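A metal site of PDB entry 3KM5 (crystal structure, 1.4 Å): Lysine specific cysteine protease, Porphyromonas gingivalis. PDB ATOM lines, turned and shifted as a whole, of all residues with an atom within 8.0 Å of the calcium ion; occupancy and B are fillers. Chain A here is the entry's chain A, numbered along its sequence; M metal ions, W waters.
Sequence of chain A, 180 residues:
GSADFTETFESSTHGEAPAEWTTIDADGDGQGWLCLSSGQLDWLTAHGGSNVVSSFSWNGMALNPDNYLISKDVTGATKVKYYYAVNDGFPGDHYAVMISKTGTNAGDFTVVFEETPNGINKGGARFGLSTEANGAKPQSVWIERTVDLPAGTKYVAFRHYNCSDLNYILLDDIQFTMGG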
ATOM      1  N   ILE A  24      17.659  16.971 -23.608  1.00  0.00           N
ATOM      2  CA  ILE A  24      17.651  17.023 -22.146  1.00  0.00           C
ATOM      3  C   ILE A  24      19.013  16.583 -21.600  1.00  0.00           C
ATOM      4  O   ILE A  24      19.522  15.486 -21.950  1.00  0.00           O
ATOM      5  CB  ILE A  24      16.543  16.146 -21.505  1.00  0.00           C
ATOM      6  CG1 ILE A  24      15.175  16.430 -22.115  1.00  0.00           C
ATOM      7  CG2 ILE A  24      16.505  16.374 -19.974  1.00  0.00           C
ATOM      8  CD1 ILE A  24      14.087  15.462 -21.642  1.00  0.00           C
ATOM      9  N   ASP A  25      19.617  17.434 -20.794  1.00  0.00           N
ATOM     10  CA  ASP A  25      20.808  17.071 -20.005  1.00  0.00           C
ATOM     11  C   ASP A  25      20.329  16.553 -18.649  1.00  0.00           C
ATOM     12  O   ASP A  25      20.376  17.303 -17.682  1.00  0.00           O
ATOM     13  CB  ASP A  25      21.667  18.322 -19.829  1.00  0.00           C
ATOM     14  CG  ASP A  25      22.821  18.132 -18.875  1.00  0.00           C
ATOM     15  OD1 ASP A  25      23.325  16.988 -18.752  1.00  0.00           O
ATOM     16  OD2 ASP A  25      23.235  19.116 -18.242  1.00  0.00           O
ATOM     17  N   ALA A  26      19.778  15.339 -18.583  1.00  0.00           N
ATOM     18  CA  ALA A  26      19.088  14.928 -17.379  1.00  0.00           C
ATOM     19  C   ALA A  26      20.034  14.704 -16.201  1.00  0.00           C
ATOM     20  O   ALA A  26      19.612  14.926 -15.061  1.00  0.00           O
ATOM     21  CB  ALA A  26      18.259  13.677 -17.679  1.00  0.00           C
ATOM     22  N   ASP A  27      21.287  14.314 -16.433  1.00  0.00           N
ATOM     23  CA  ASP A  27      22.220  14.151 -15.309  1.00  0.00           C
ATOM     24  C   ASP A  27      22.671  15.505 -14.768  1.00  0.00           C
ATOM     25  O   ASP A  27      23.140  15.584 -13.624  1.00  0.00           O
ATOM     26  CB  ASP A  27      23.435  13.364 -15.732  1.00  0.00           C
ATOM     27  CG  ASP A  27      24.112  13.976 -16.937  1.00  0.00           C
ATOM     28  OD1 ASP A  27      23.555  13.887 -18.050  1.00  0.00           O
ATOM     29  OD2 ASP A  27      25.132  14.610 -16.762  1.00  0.00           O
ATOM     30  N   GLY A  28      22.574  16.567 -15.580  1.00  0.00           N
ATOM     31  CA  GLY A  28      22.893  17.916 -15.093  1.00  0.00           C
ATOM     32  C   GLY A  28      24.309  18.379 -15.160  1.00  0.00           C
ATOM     33  O   GLY A  28      24.647  19.379 -14.506  1.00  0.00           O
ATOM     34  N   ASP A  29      25.182  17.743 -15.938  1.00  0.00           N
ATOM     35  CA  ASP A  29      26.579  18.138 -16.022  1.00  0.00           C
ATOM     36  C   ASP A  29      26.915  19.179 -17.127  1.00  0.00           C
ATOM     37  O   ASP A  29      28.067  19.460 -17.404  1.00  0.00           O
ATOM     38  CB  ASP A  29      27.523  16.931 -16.207  1.00  0.00           C
ATOM     39  CG  ASP A  29      27.399  16.263 -17.554  1.00  0.00           C
ATOM     40  OD1 ASP A  29      26.543  16.702 -18.368  1.00  0.00           O
ATOM     41  OD2 ASP A  29      28.143  15.297 -17.795  1.00  0.00           O
ATOM     42  N   GLY A  30      25.904  19.743 -17.789  1.00  0.00           N
ATOM     43  CA  GLY A  30      26.176  20.770 -18.810  1.00  0.00           C
ATOM     44  C   GLY A  30      26.795  20.244 -20.091  1.00  0.00           C
ATOM     45  O   GLY A  30      27.312  20.999 -20.904  1.00  0.00           O
ATOM     46  N   GLN A  31      26.686  18.937 -20.305  1.00  0.00           N
ATOM     47  CA  GLN A  31      27.202  18.249 -21.496  1.00  0.00           C
ATOM     48  C   GLN A  31      26.108  17.324 -22.038  1.00  0.00           C
ATOM     49  O   GLN A  31      25.482  16.577 -21.276  1.00  0.00           O
ATOM     50  CB  GLN A  31      28.478  17.457 -21.164  1.00  0.00           C
ATOM     51  CG  GLN A  31      29.583  18.401 -20.599  1.00  0.00           C
ATOM     52  CD  GLN A  31      30.900  17.784 -20.280  1.00  0.00           C
ATOM     53  OE1 GLN A  31      31.388  17.859 -19.141  1.00  0.00           O
ATOM     54  NE2 GLN A  31      31.520  17.184 -21.273  1.00  0.00           N
ATOM     55  N   GLY A  32      25.845  17.403 -23.351  1.00  0.00           N
ATOM     56  CA  GLY A  32      24.753  16.647 -23.893  1.00  0.00           C
ATOM     57  C   GLY A  32      24.989  16.372 -25.363  1.00  0.00           C
ATOM     58  O   GLY A  32      26.145  16.328 -25.814  1.00  0.00           O
ATOM     59  N   TRP A  33      23.891  16.146 -26.078  1.00  0.00           N
ATOM     60  CA  TRP A  33      23.956  15.859 -27.507  1.00  0.00           C
ATOM     61  C   TRP A  33      24.286  17.113 -28.330  1.00  0.00           C
ATOM     62  O   TRP A  33      23.624  18.142 -28.181  1.00  0.00           O
ATOM     63  CB  TRP A  33      22.627  15.305 -27.979  1.00  0.00           C
ATOM     64  CG  TRP A  33      22.316  13.909 -27.526  1.00  0.00           C
ATOM     65  CD1 TRP A  33      21.525  13.575 -26.474  1.00  0.00           C
ATOM     66  CD2 TRP A  33      22.731  12.669 -28.110  1.00  0.00           C
ATOM     67  NE1 TRP A  33      21.421  12.230 -26.378  1.00  0.00           N
ATOM     68  CE2 TRP A  33      22.173  11.633 -27.353  1.00  0.00           C
ATOM     69  CE3 TRP A  33      23.563  12.345 -29.185  1.00  0.00           C
ATOM     70  CZ2 TRP A  33      22.337  10.280 -27.697  1.00  0.00           C
ATOM     71  CZ3 TRP A  33      23.757  11.002 -29.503  1.00  0.00           C
ATOM     72  CH2 TRP A  33      23.166   9.996 -28.734  1.00  0.00           C
ATOM     73  N   SER A  55      27.241  12.282 -28.330  1.00  0.00           N
ATOM     74  CA  SER A  55      27.168  12.405 -26.886  1.00  0.00           C
ATOM     75  C   SER A  55      28.366  11.635 -26.276  1.00  0.00           C
ATOM     76  O   SER A  55      28.726  10.562 -26.721  1.00  0.00           O
ATOM     77  CB  SER A  55      25.828  11.856 -26.370  1.00  0.00           C
ATOM     78  OG  SER A  55      25.764  11.931 -24.934  1.00  0.00           O
ATOM     79  N   PHE A  56      29.000  12.238 -25.298  1.00  0.00           N
ATOM     80  CA  PHE A  56      30.247  11.736 -24.739  1.00  0.00           C
ATOM     81  C   PHE A  56      30.094  11.126 -23.323  1.00  0.00           C
ATOM     82  O   PHE A  56      29.381  11.652 -22.459  1.00  0.00           O
ATOM     83  CB  PHE A  56      31.302  12.863 -24.720  1.00  0.00           C
ATOM     84  CG  PHE A  56      31.732  13.259 -26.087  1.00  0.00           C
ATOM     85  CD1 PHE A  56      32.876  12.725 -26.648  1.00  0.00           C
ATOM     86  CD2 PHE A  56      30.972  14.109 -26.853  1.00  0.00           C
ATOM     87  CE1 PHE A  56      33.277  13.074 -27.896  1.00  0.00           C
ATOM     88  CE2 PHE A  56      31.347  14.469 -28.127  1.00  0.00           C
ATOM     89  CZ  PHE A  56      32.505  13.931 -28.669  1.00  0.00           C
ATOM     90  N   LEU A  63      32.794  11.225 -17.713  1.00  0.00           N
ATOM     91  CA  LEU A  63      31.399  11.682 -17.548  1.00  0.00           C
ATOM     92  C   LEU A  63      30.478  10.510 -17.244  1.00  0.00           C
ATOM     93  O   LEU A  63      30.819   9.365 -17.553  1.00  0.00           O
ATOM     94  CB  LEU A  63      30.903  12.378 -18.813  1.00  0.00           C
ATOM     95  CG  LEU A  63      31.760  13.534 -19.298  1.00  0.00           C
ATOM     96  CD1 LEU A  63      31.385  14.029 -20.709  1.00  0.00           C
ATOM     97  CD2 LEU A  63      31.747  14.675 -18.297  1.00  0.00           C
ATOM     98  N   ASN A  64      29.328  10.829 -16.665  1.00  0.00           N
ATOM     99  CA  ASN A  64      28.254   9.920 -16.301  1.00  0.00           C
ATOM    100  C   ASN A  64      26.949  10.428 -16.956  1.00  0.00           C
ATOM    101  O   ASN A  64      26.079  11.038 -16.302  1.00  0.00           O
ATOM    102  CB  ASN A  64      28.083   9.857 -14.770  1.00  0.00           C
ATOM    103  CG  ASN A  64      29.138   8.986 -14.108  1.00  0.00           C
ATOM    104  OD1 ASN A  64      30.326   9.341 -14.079  1.00  0.00           O
ATOM    105  ND2 ASN A  64      28.693   7.852 -13.562  1.00  0.00           N
ATOM    106  N   PRO A  65      26.853  10.247 -18.281  1.00  0.00           N
ATOM    107  CA  PRO A  65      25.729  10.895 -18.956  1.00  0.00           C
ATOM    108  C   PRO A  65      24.356  10.310 -18.687  1.00  0.00           C
ATOM    109  O   PRO A  65      24.193   9.137 -18.351  1.00  0.00           O
ATOM    110  CB  PRO A  65      26.063  10.655 -20.443  1.00  0.00           C
ATOM    111  CG  PRO A  65      26.904   9.408 -20.435  1.00  0.00           C
ATOM    112  CD  PRO A  65      27.760   9.611 -19.244  1.00  0.00           C
ATOM    113  N   ASP A  66      23.358  11.167 -18.826  1.00  0.00           N
ATOM    114  CA  ASP A  66      21.963  10.785 -19.010  1.00  0.00           C
ATOM    115  C   ASP A  66      21.341  11.838 -19.918  1.00  0.00           C
ATOM    116  O   ASP A  66      20.671  12.776 -19.467  1.00  0.00           O
ATOM    117  CB  ASP A  66      21.231  10.612 -17.671  1.00  0.00           C
ATOM    118  CG  ASP A  66      19.830  10.033 -17.849  1.00  0.00           C
ATOM    119  OD1 ASP A  66      19.462   9.707 -18.987  1.00  0.00           O
ATOM    120  OD2 ASP A  66      19.042   9.973 -16.873  1.00  0.00           O
ATOM    121  N   ASN A  67      21.655  11.690 -21.199  1.00  0.00           N
ATOM    122  CA  ASN A  67      21.395  12.712 -22.192  1.00  0.00           C
ATOM    123  C   ASN A  67      20.340  12.227 -23.175  1.00  0.00           C
ATOM    124  O   ASN A  67      20.478  11.157 -23.777  1.00  0.00           O
ATOM    125  CB  ASN A  67      22.667  13.055 -22.998  1.00  0.00           C
ATOM    126  CG  ASN A  67      23.817  13.508 -22.144  1.00  0.00           C
ATOM    127  OD1 ASN A  67      23.625  14.117 -21.100  1.00  0.00           O
ATOM    128  ND2 ASN A  67      25.034  13.318 -22.651  1.00  0.00           N
ATOM    129  N   TYR A  68      19.258  13.003 -23.331  1.00  0.00           N
ATOM    130  CA  TYR A  68      18.189  12.681 -24.292  1.00  0.00           C
ATOM    131  C   TYR A  68      18.254  13.560 -25.533  1.00  0.00           C
ATOM    132  O   TYR A  68      18.361  14.774 -25.449  1.00  0.00           O
ATOM    133  CB  TYR A  68      16.806  12.894 -23.638  1.00  0.00           C
ATOM    134  CG  TYR A  68      16.406  11.991 -22.483  1.00  0.00           C
ATOM    135  CD1 TYR A  68      15.336  11.089 -22.606  1.00  0.00           C
ATOM    136  CD2 TYR A  68      17.010  12.128 -21.273  1.00  0.00           C
ATOM    137  CE1 TYR A  68      14.927  10.318 -21.544  1.00  0.00           C
ATOM    138  CE2 TYR A  68      16.591  11.340 -20.196  1.00  0.00           C
ATOM    139  CZ  TYR A  68      15.558  10.455 -20.350  1.00  0.00           C
ATOM    140  OH  TYR A  68      15.173   9.699 -19.246  1.00  0.00           O
ATOM    141  N   HIS A 160      21.569   8.447 -24.102  1.00  0.00           N
ATOM    142  CA  HIS A 160      22.904   7.949 -23.769  1.00  0.00           C
ATOM    143  C   HIS A 160      22.979   7.975 -22.253  1.00  0.00           C
ATOM    144  O   HIS A 160      22.933   9.041 -21.619  1.00  0.00           O
ATOM    145  CB  HIS A 160      23.972   8.858 -24.419  1.00  0.00           C
ATOM    146  CG  HIS A 160      25.401   8.473 -24.171  1.00  0.00           C
ATOM    147  ND1 HIS A 160      26.411   9.408 -24.210  1.00  0.00           N
ATOM    148  CD2 HIS A 160      25.995   7.271 -23.943  1.00  0.00           C
ATOM    149  CE1 HIS A 160      27.570   8.791 -24.083  1.00  0.00           C
ATOM    150  NE2 HIS A 160      27.354   7.506 -23.896  1.00  0.00           N
HETATM  151 CA    CA M   1      24.828  15.412 -19.437  1.00  0.00          CA
HETATM  152  O   HOH W   1      26.752  13.917 -19.653  1.00  0.00           O
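Within 4 Å of the calcium ion: Asp 25, Asp 27, Asp 29, Gln 31 and Asn 67.
O of Gln 31 is bound to the calcium ion, at 2.3 Å.
The calcium ion is bound by OD1 of Asp 25 (2.3 Å).
The side-chain carboxylate (OD1) of Asp 29 is bound to the calcium ion (2.4 Å).
OD1 of Asp 27 is bound to the calcium ion.
OD1 of Asn 67 binds the calcium ion (2.4 Å).
Water W1 binds the calcium ion (2.4 Å).
The side-chain carboxylate (OD2) of Asp 27 binds the calcium ion (2.8 Å).
The calcium ion has seven donor atoms within binding distance.
The backbone NH (N) of Asp 27 sits at hydrogen-bond distance from the backbone carbonyl oxygen (O) of Asp 66 (3.5 Å).
The indole nitrogen (NE1) of Trp 33 is in hydrogen-bond range of the backbone carbonyl oxygen (O) of Asn 67.
The side-chain hydroxyl (OG) of Ser 55 sits at hydrogen-bond distance from the side-chain amide nitrogen (ND2) of Asn 67, at 2.8 Å.
OD1 of Asp 25 sits close to N of Gly 28.
The backbone NH (N) of Gly 30 is in hydrogen-bond range of the side-chain carboxylate (OD2) of Asp 25 (2.8 Å).
The backbone carbonyl oxygen of Asn 67 sits at hydrogen-bond distance from the backbone NH of His 160 (2.9 Å).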
